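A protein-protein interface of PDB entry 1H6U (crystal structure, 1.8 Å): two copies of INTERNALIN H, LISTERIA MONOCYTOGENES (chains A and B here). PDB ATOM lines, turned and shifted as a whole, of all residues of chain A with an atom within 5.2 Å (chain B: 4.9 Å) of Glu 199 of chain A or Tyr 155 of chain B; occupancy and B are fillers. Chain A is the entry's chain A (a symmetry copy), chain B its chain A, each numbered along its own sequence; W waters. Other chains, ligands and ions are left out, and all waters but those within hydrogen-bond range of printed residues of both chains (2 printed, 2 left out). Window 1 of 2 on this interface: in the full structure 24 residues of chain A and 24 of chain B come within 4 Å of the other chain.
O of Gln 132 of chain B is in hydrogen-bond range of N of Tyr 155 of chain B (2.9 Å).
The backbone carbonyl oxygen (O) of Leu 156 of chain B lies within hydrogen-bond range of the backbone NH (N) of Lys 179 of chain B, at 2.9 Å.
N of Leu 178 of chain A is in hydrogen-bond range of O of Glu 199 of chain A (2.8 Å).
O of Ile 198 of chain A sits at hydrogen-bond distance from N of Phe 220 of chain A (2.8 Å).
N of Ile 221 of chain A is in hydrogen-bond range of O of Ile 198 of chain A, 3.0 Å away.
A ring nitrogen (NE2) of His 201 of chain A is in hydrogen-bond range of the side-chain carboxylate (OE2) of Glu 199 of chain A, 2.5 Å away.
Among the printed residues, merely in contact across the chains: Phe 220 of chain A with Tyr 135 of chain B (3.2 Å), Ile 198 of chain A with Val 133 of chain B (3.5 Å), Ile 198 of chain A with Tyr 135 of chain B (3.5 Å), Ile 221 of chain A with Lys 179 of chain B (3.8 Å), Ile 221 of chain A with Tyr 155 of chain B (3.8 Å) and Ile 198 of chain A with Tyr 155 of chain B (3.9 Å).
Positions printed for both chains: 177, 179 and 199.
Of the 7 pairs that touch across the chains among the printed residues, none has its exchanged pair printed and touching as well.
The side-chain hydroxyl of Tyr 155 of chain B sits at hydrogen-bond distance from the side-chain carboxylate of Glu 199 of chain A (3.4 Å).
Of the printed residues of chain B, Glu 199 of chain A touches Tyr 155 (3.4 Å).
Printed residues of chain A within 4 Å of Tyr 135 of chain B: Ile 198 (3.5 Å) and Phe 220 (3.2 Å).
Of the printed residues of chain B, Ile 221 of chain A touches Tyr 155 and Lys 179.
Of the printed residues of chain A, Val 133 of chain B touches Ile 198.
Of the printed residues of chain B, Ile 198 of chain A touches Val 133, Tyr 135 and Tyr 155.
Of the printed residues of chain B, Phe 220 of chain A touches Tyr 135.
The nearest printed residue of chain B that does not touch Glu 199 of chain A is Glu 199 of chain B (4.6 Å).
Of the 13 printed residues of chain B, 4 touch a printed residue of chain A.
Among the printed residues, 7 pairs touch across the chains.
Water W1 lies within hydrogen-bond range of OE2 of Glu 199 of chain B (2.5 Å), NZ of Lys 179 of chain B (2.8 Å) and OE1 of Glu 199 of chain A (2.8 Å).
Water W2 lies within hydrogen-bond range of OE2 of Glu 199 of chain A (2.5 Å), NZ of Lys 179 of chain A (2.8 Å) and OE1 of Glu 199 of chain B (2.8 Å).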
ATOM      1  N   THR A 176     -28.272  11.602 -18.790  1.00  0.00           N
ATOM      2  CA  THR A 176     -27.462  10.632 -18.135  1.00  0.00           C
ATOM      3  C   THR A 176     -26.007  10.692 -18.542  1.00  0.00           C
ATOM      4  O   THR A 176     -25.181  10.245 -17.820  1.00  0.00           O
ATOM      5  CB  THR A 176     -27.993   9.195 -18.284  1.00  0.00           C
ATOM      6  OG1 THR A 176     -28.133   8.776 -19.642  1.00  0.00           O
ATOM      7  CG2 THR A 176     -29.330   9.038 -17.595  1.00  0.00           C
ATOM      8  N   THR A 177     -25.732  11.081 -19.776  1.00  0.00           N
ATOM      9  CA  THR A 177     -24.359  11.188 -20.265  1.00  0.00           C
ATOM     10  C   THR A 177     -24.150  12.604 -20.803  1.00  0.00           C
ATOM     11  O   THR A 177     -24.932  13.109 -21.664  1.00  0.00           O
ATOM     12  CB  THR A 177     -24.085  10.181 -21.340  1.00  0.00           C
ATOM     13  OG1 THR A 177     -23.991   8.853 -20.810  1.00  0.00           O
ATOM     14  CG2 THR A 177     -22.711  10.438 -21.933  1.00  0.00           C
ATOM     15  N   LEU A 178     -23.198  13.311 -20.228  1.00  0.00           N
ATOM     16  CA  LEU A 178     -22.791  14.622 -20.709  1.00  0.00           C
ATOM     17  C   LEU A 178     -21.332  14.629 -21.044  1.00  0.00           C
ATOM     18  O   LEU A 178     -20.508  14.490 -20.170  1.00  0.00           O
ATOM     19  CB  LEU A 178     -23.058  15.702 -19.688  1.00  0.00           C
ATOM     20  CG  LEU A 178     -22.579  17.080 -19.975  1.00  0.00           C
ATOM     21  CD1 LEU A 178     -23.224  17.688 -21.273  1.00  0.00           C
ATOM     22  CD2 LEU A 178     -22.773  18.027 -18.795  1.00  0.00           C
ATOM     23  N   LYS A 179     -21.014  14.853 -22.314  1.00  0.00           N
ATOM     24  CA  LYS A 179     -19.652  14.920 -22.769  1.00  0.00           C
ATOM     25  C   LYS A 179     -19.326  16.356 -23.195  1.00  0.00           C
ATOM     26  O   LYS A 179     -19.880  16.890 -24.150  1.00  0.00           O
ATOM     27  CB  LYS A 179     -19.420  13.898 -23.869  1.00  0.00           C
ATOM     28  CG  LYS A 179     -19.640  12.501 -23.365  1.00  0.00           C
ATOM     29  CD  LYS A 179     -19.972  11.482 -24.448  1.00  0.00           C
ATOM     30  CE  LYS A 179     -18.735  11.067 -25.133  1.00  0.00           C
ATOM     31  NZ  LYS A 179     -18.414   9.704 -24.893  1.00  0.00           N
ATOM     32  N   LEU A 197     -27.437  11.940 -13.823  1.00  0.00           N
ATOM     33  CA  LEU A 197     -26.207  11.974 -14.546  1.00  0.00           C
ATOM     34  C   LEU A 197     -25.372  10.736 -14.146  1.00  0.00           C
ATOM     35  O   LEU A 197     -25.128  10.552 -12.994  1.00  0.00           O
ATOM     36  CB  LEU A 197     -25.371  13.196 -14.289  1.00  0.00           C
ATOM     37  CG  LEU A 197     -25.807  14.508 -14.892  1.00  0.00           C
ATOM     38  CD1 LEU A 197     -24.835  15.546 -14.380  1.00  0.00           C
ATOM     39  CD2 LEU A 197     -25.736  14.377 -16.341  1.00  0.00           C
ATOM     40  N   ILE A 198     -24.936   9.969 -15.135  1.00  0.00           N
ATOM     41  CA  ILE A 198     -24.100   8.780 -14.919  1.00  0.00           C
ATOM     42  C   ILE A 198     -22.671   9.036 -15.287  1.00  0.00           C
ATOM     43  O   ILE A 198     -21.727   8.599 -14.583  1.00  0.00           O
ATOM     44  CB  ILE A 198     -24.611   7.514 -15.743  1.00  0.00           C
ATOM     45  CG1 ILE A 198     -26.031   7.082 -15.300  1.00  0.00           C
ATOM     46  CG2 ILE A 198     -23.553   6.419 -15.598  1.00  0.00           C
ATOM     47  CD1 ILE A 198     -26.692   6.116 -16.218  1.00  0.00           C
ATOM     48  N   GLU A 199     -22.483   9.750 -16.388  1.00  0.00           N
ATOM     49  CA  GLU A 199     -21.199  10.026 -16.960  1.00  0.00           C
ATOM     50  C   GLU A 199     -21.105  11.509 -17.345  1.00  0.00           C
ATOM     51  O   GLU A 199     -21.924  12.013 -18.089  1.00  0.00           O
ATOM     52  CB  GLU A 199     -21.033   9.143 -18.203  1.00  0.00           C
ATOM     53  CG  GLU A 199     -19.686   9.109 -18.873  1.00  0.00           C
ATOM     54  CD  GLU A 199     -19.587   8.039 -19.958  1.00  0.00           C
ATOM     55  OE1 GLU A 199     -20.246   6.946 -19.889  1.00  0.00           O
ATOM     56  OE2 GLU A 199     -18.887   8.320 -20.880  1.00  0.00           O
ATOM     57  N   VAL A 200     -20.074  12.164 -16.881  1.00  0.00           N
ATOM     58  CA  VAL A 200     -19.822  13.572 -17.120  1.00  0.00           C
ATOM     59  C   VAL A 200     -18.365  13.744 -17.447  1.00  0.00           C
ATOM     60  O   VAL A 200     -17.469  13.431 -16.635  1.00  0.00           O
ATOM     61  CB  VAL A 200     -20.083  14.374 -15.860  1.00  0.00           C
ATOM     62  CG1 VAL A 200     -19.766  15.791 -16.073  1.00  0.00           C
ATOM     63  CG2 VAL A 200     -21.552  14.315 -15.408  1.00  0.00           C
ATOM     64  N   HIS A 201     -18.103  14.282 -18.615  1.00  0.00           N
ATOM     65  CA  HIS A 201     -16.736  14.508 -19.082  1.00  0.00           C
ATOM     66  C   HIS A 201     -16.494  16.014 -19.151  1.00  0.00           C
ATOM     67  O   HIS A 201     -17.126  16.716 -19.945  1.00  0.00           O
ATOM     68  CB  HIS A 201     -16.525  13.832 -20.493  1.00  0.00           C
ATOM     69  CG  HIS A 201     -16.646  12.327 -20.484  1.00  0.00           C
ATOM     70  ND1 HIS A 201     -15.551  11.494 -20.606  1.00  0.00           N
ATOM     71  CD2 HIS A 201     -17.720  11.511 -20.325  1.00  0.00           C
ATOM     72  CE1 HIS A 201     -15.945  10.235 -20.533  1.00  0.00           C
ATOM     73  NE2 HIS A 201     -17.259  10.214 -20.377  1.00  0.00           N
ATOM     74  N   LEU A 219     -23.940   9.044 -10.338  1.00  0.00           N
ATOM     75  CA  LEU A 219     -22.726   9.481 -11.033  1.00  0.00           C
ATOM     76  C   LEU A 219     -21.596   8.517 -10.852  1.00  0.00           C
ATOM     77  O   LEU A 219     -21.210   8.266  -9.722  1.00  0.00           O
ATOM     78  CB  LEU A 219     -22.329  10.843 -10.568  1.00  0.00           C
ATOM     79  CG  LEU A 219     -21.141  11.495 -11.326  1.00  0.00           C
ATOM     80  CD1 LEU A 219     -21.459  11.758 -12.810  1.00  0.00           C
ATOM     81  CD2 LEU A 219     -20.770  12.811 -10.619  1.00  0.00           C
ATOM     82  N   PHE A 220     -21.128   7.922 -11.961  1.00  0.00           N
ATOM     83  CA  PHE A 220     -20.110   6.908 -11.901  1.00  0.00           C
ATOM     84  C   PHE A 220     -18.852   7.198 -12.674  1.00  0.00           C
ATOM     85  O   PHE A 220     -17.833   6.622 -12.353  1.00  0.00           O
ATOM     86  CB  PHE A 220     -20.644   5.522 -12.273  1.00  0.00           C
ATOM     87  CG  PHE A 220     -21.694   5.003 -11.286  1.00  0.00           C
ATOM     88  CD1 PHE A 220     -21.297   4.303 -10.145  1.00  0.00           C
ATOM     89  CD2 PHE A 220     -23.041   5.140 -11.560  1.00  0.00           C
ATOM     90  CE1 PHE A 220     -22.165   3.884  -9.254  1.00  0.00           C
ATOM     91  CE2 PHE A 220     -24.016   4.695 -10.637  1.00  0.00           C
ATOM     92  CZ  PHE A 220     -23.582   4.064  -9.454  1.00  0.00           C
ATOM     93  N   ILE A 221     -18.908   8.038 -13.699  1.00  0.00           N
ATOM     94  CA  ILE A 221     -17.748   8.408 -14.488  1.00  0.00           C
ATOM     95  C   ILE A 221     -17.732   9.923 -14.542  1.00  0.00           C
ATOM     96  O   ILE A 221     -18.772  10.525 -14.801  1.00  0.00           O
ATOM     97  CB  ILE A 221     -17.819   7.873 -15.912  1.00  0.00           C
ATOM     98  CG1 ILE A 221     -17.582   6.342 -15.942  1.00  0.00           C
ATOM     99  CG2 ILE A 221     -16.787   8.515 -16.844  1.00  0.00           C
ATOM    100  CD1 ILE A 221     -17.896   5.755 -17.364  1.00  0.00           C
ATOM    101  N   GLN B 132     -32.388   0.310 -14.035  1.00  0.00           N
ATOM    102  CA  GLN B 132     -31.988   1.079 -15.235  1.00  0.00           C
ATOM    103  C   GLN B 132     -30.495   1.072 -15.441  1.00  0.00           C
ATOM    104  O   GLN B 132     -30.067   1.149 -16.560  1.00  0.00           O
ATOM    105  CB  GLN B 132     -32.355   2.541 -15.063  1.00  0.00           C
ATOM    106  CG  GLN B 132     -33.911   2.731 -15.001  1.00  0.00           C
ATOM    107  CD  GLN B 132     -34.350   4.180 -14.805  1.00  0.00           C
ATOM    108  OE1 GLN B 132     -33.552   5.037 -14.469  1.00  0.00           O
ATOM    109  NE2 GLN B 132     -35.612   4.426 -14.947  1.00  0.00           N
ATOM    110  N   VAL B 133     -29.761   1.055 -14.346  1.00  0.00           N
ATOM    111  CA  VAL B 133     -28.275   1.082 -14.414  1.00  0.00           C
ATOM    112  C   VAL B 133     -27.726  -0.059 -13.542  1.00  0.00           C
ATOM    113  O   VAL B 133     -27.956  -0.086 -12.300  1.00  0.00           O
ATOM    114  CB  VAL B 133     -27.730   2.410 -13.872  1.00  0.00           C
ATOM    115  CG1 VAL B 133     -26.194   2.488 -13.978  1.00  0.00           C
ATOM    116  CG2 VAL B 133     -28.371   3.572 -14.531  1.00  0.00           C
ATOM    117  N   LEU B 134     -26.898  -0.916 -14.122  1.00  0.00           N
ATOM    118  CA  LEU B 134     -26.371  -2.058 -13.395  1.00  0.00           C
ATOM    119  C   LEU B 134     -24.891  -2.280 -13.733  1.00  0.00           C
ATOM    120  O   LEU B 134     -24.549  -2.388 -14.888  1.00  0.00           O
ATOM    121  CB  LEU B 134     -27.131  -3.302 -13.725  1.00  0.00           C
ATOM    122  CG  LEU B 134     -26.777  -4.634 -13.117  1.00  0.00           C
ATOM    123  CD1 LEU B 134     -26.781  -4.626 -11.596  1.00  0.00           C
ATOM    124  CD2 LEU B 134     -27.703  -5.726 -13.649  1.00  0.00           C
ATOM    125  N   TYR B 135     -24.114  -2.362 -12.672  1.00  0.00           N
ATOM    126  CA  TYR B 135     -22.710  -2.747 -12.794  1.00  0.00           C
ATOM    127  C   TYR B 135     -22.510  -4.116 -12.154  1.00  0.00           C
ATOM    128  O   TYR B 135     -22.713  -4.284 -10.965  1.00  0.00           O
ATOM    129  CB  TYR B 135     -21.813  -1.765 -12.077  1.00  0.00           C
ATOM    130  CG  TYR B 135     -21.925  -0.370 -12.592  1.00  0.00           C
ATOM    131  CD1 TYR B 135     -22.934   0.475 -12.166  1.00  0.00           C
ATOM    132  CD2 TYR B 135     -21.017   0.119 -13.521  1.00  0.00           C
ATOM    133  CE1 TYR B 135     -22.993   1.813 -12.663  1.00  0.00           C
ATOM    134  CE2 TYR B 135     -21.144   1.406 -14.058  1.00  0.00           C
ATOM    135  CZ  TYR B 135     -22.112   2.213 -13.636  1.00  0.00           C
ATOM    136  OH  TYR B 135     -22.206   3.499 -14.179  1.00  0.00           O
ATOM    137  N   LEU B 153     -33.809  -1.754 -18.261  1.00  0.00           N
ATOM    138  CA  LEU B 153     -32.393  -1.548 -18.227  1.00  0.00           C
ATOM    139  C   LEU B 153     -31.898  -0.634 -19.357  1.00  0.00           C
ATOM    140  O   LEU B 153     -32.206  -0.854 -20.516  1.00  0.00           O
ATOM    141  CB  LEU B 153     -31.674  -2.912 -18.188  1.00  0.00           C
ATOM    142  CG  LEU B 153     -30.294  -3.023 -17.548  1.00  0.00           C
ATOM    143  CD1 LEU B 153     -30.211  -2.580 -16.086  1.00  0.00           C
ATOM    144  CD2 LEU B 153     -29.818  -4.512 -17.726  1.00  0.00           C
ATOM    145  N   GLN B 154     -31.086   0.357 -19.004  1.00  0.00           N
ATOM    146  CA  GLN B 154     -30.585   1.312 -19.966  1.00  0.00           C
ATOM    147  C   GLN B 154     -29.052   1.255 -20.076  1.00  0.00           C
ATOM    148  O   GLN B 154     -28.480   1.489 -21.136  1.00  0.00           O
ATOM    149  CB  GLN B 154     -30.956   2.721 -19.536  1.00  0.00           C
ATOM    150  CG  GLN B 154     -32.380   3.059 -19.969  1.00  0.00           C
ATOM    151  CD  GLN B 154     -33.072   4.243 -19.253  1.00  0.00           C
ATOM    152  OE1 GLN B 154     -33.051   4.327 -18.026  1.00  0.00           O
ATOM    153  NE2 GLN B 154     -33.821   5.066 -20.024  1.00  0.00           N
ATOM    154  N   TYR B 155     -28.418   0.959 -18.962  1.00  0.00           N
ATOM    155  CA  TYR B 155     -26.940   1.005 -18.869  1.00  0.00           C
ATOM    156  C   TYR B 155     -26.529  -0.282 -18.170  1.00  0.00           C
ATOM    157  O   TYR B 155     -26.832  -0.483 -16.998  1.00  0.00           O
ATOM    158  CB  TYR B 155     -26.570   2.237 -18.032  1.00  0.00           C
ATOM    159  CG  TYR B 155     -25.149   2.711 -18.123  1.00  0.00           C
ATOM    160  CD1 TYR B 155     -24.832   3.861 -18.822  1.00  0.00           C
ATOM    161  CD2 TYR B 155     -24.168   2.065 -17.456  1.00  0.00           C
ATOM    162  CE1 TYR B 155     -23.523   4.324 -18.896  1.00  0.00           C
ATOM    163  CE2 TYR B 155     -22.821   2.508 -17.559  1.00  0.00           C
ATOM    164  CZ  TYR B 155     -22.523   3.652 -18.239  1.00  0.00           C
ATOM    165  OH  TYR B 155     -21.177   4.095 -18.281  1.00  0.00           O
ATOM    166  N   LEU B 156     -25.791  -1.144 -18.860  1.00  0.00           N
ATOM    167  CA  LEU B 156     -25.323  -2.411 -18.326  1.00  0.00           C
ATOM    168  C   LEU B 156     -23.815  -2.568 -18.486  1.00  0.00           C
ATOM    169  O   LEU B 156     -23.339  -2.433 -19.568  1.00  0.00           O
ATOM    170  CB  LEU B 156     -25.943  -3.578 -19.037  1.00  0.00           C
ATOM    171  CG  LEU B 156     -25.531  -4.941 -18.573  1.00  0.00           C
ATOM    172  CD1 LEU B 156     -25.773  -5.029 -17.005  1.00  0.00           C
ATOM    173  CD2 LEU B 156     -26.249  -6.028 -19.353  1.00  0.00           C
ATOM    174  N   SER B 157     -23.123  -2.786 -17.407  1.00  0.00           N
ATOM    175  CA  SER B 157     -21.695  -2.952 -17.392  1.00  0.00           C
ATOM    176  C   SER B 157     -21.425  -4.310 -16.768  1.00  0.00           C
ATOM    177  O   SER B 157     -21.830  -4.584 -15.640  1.00  0.00           O
ATOM    178  CB  SER B 157     -21.117  -1.817 -16.570  1.00  0.00           C
ATOM    179  OG  SER B 157     -19.641  -1.885 -16.610  1.00  0.00           O
ATOM    180  N   LEU B 175     -31.844  -0.596 -23.731  1.00  0.00           N
ATOM    181  CA  LEU B 175     -30.408  -0.512 -23.534  1.00  0.00           C
ATOM    182  C   LEU B 175     -29.764   0.460 -24.466  1.00  0.00           C
ATOM    183  O   LEU B 175     -29.920   0.361 -25.708  1.00  0.00           O
ATOM    184  CB  LEU B 175     -29.732  -1.868 -23.741  1.00  0.00           C
ATOM    185  CG  LEU B 175     -29.391  -2.740 -22.558  1.00  0.00           C
ATOM    186  CD1 LEU B 175     -28.295  -3.729 -23.089  1.00  0.00           C
ATOM    187  CD2 LEU B 175     -28.854  -2.039 -21.390  1.00  0.00           C
ATOM    188  N   THR B 177     -26.280   1.761 -23.375  1.00  0.00           N
ATOM    189  CA  THR B 177     -24.849   1.585 -23.133  1.00  0.00           C
ATOM    190  C   THR B 177     -24.620   0.158 -22.633  1.00  0.00           C
ATOM    191  O   THR B 177     -25.264  -0.311 -21.647  1.00  0.00           O
ATOM    192  CB  THR B 177     -24.343   2.573 -22.126  1.00  0.00           C
ATOM    193  OG1 THR B 177     -24.278   3.897 -22.670  1.00  0.00           O
ATOM    194  CG2 THR B 177     -22.901   2.246 -21.781  1.00  0.00           C
ATOM    195  N   LYS B 179     -21.382  -2.249 -21.683  1.00  0.00           N
ATOM    196  CA  LYS B 179     -19.967  -2.385 -21.472  1.00  0.00           C
ATOM    197  C   LYS B 179     -19.643  -3.837 -21.104  1.00  0.00           C
ATOM    198  O   LYS B 179     -20.048  -4.347 -20.064  1.00  0.00           O
ATOM    199  CB  LYS B 179     -19.497  -1.381 -20.434  1.00  0.00           C
ATOM    200  CG  LYS B 179     -19.733   0.029 -20.898  1.00  0.00           C
ATOM    201  CD  LYS B 179     -19.819   1.057 -19.779  1.00  0.00           C
ATOM    202  CE  LYS B 179     -18.463   1.409 -19.322  1.00  0.00           C
ATOM    203  NZ  LYS B 179     -18.122   2.755 -19.620  1.00  0.00           N
ATOM    204  N   GLU B 199     -23.610   2.946 -27.284  1.00  0.00           N
ATOM    205  CA  GLU B 199     -22.261   2.604 -26.943  1.00  0.00           C
ATOM    206  C   GLU B 199     -22.175   1.117 -26.574  1.00  0.00           C
ATOM    207  O   GLU B 199     -22.876   0.651 -25.697  1.00  0.00           O
ATOM    208  CB  GLU B 199     -21.838   3.474 -25.753  1.00  0.00           C
ATOM    209  CG  GLU B 199     -20.394   3.438 -25.328  1.00  0.00           C
ATOM    210  CD  GLU B 199     -20.055   4.496 -24.281  1.00  0.00           C
ATOM    211  OE1 GLU B 199     -20.662   5.621 -24.239  1.00  0.00           O
ATOM    212  OE2 GLU B 199     -19.219   4.177 -23.494  1.00  0.00           O
HETATM  213  O   HOH W   1     -18.687   4.977 -21.227  1.00  0.00           O
HETATM  214  O   HOH W   2     -18.798   7.504 -23.202  1.00  0.00           O
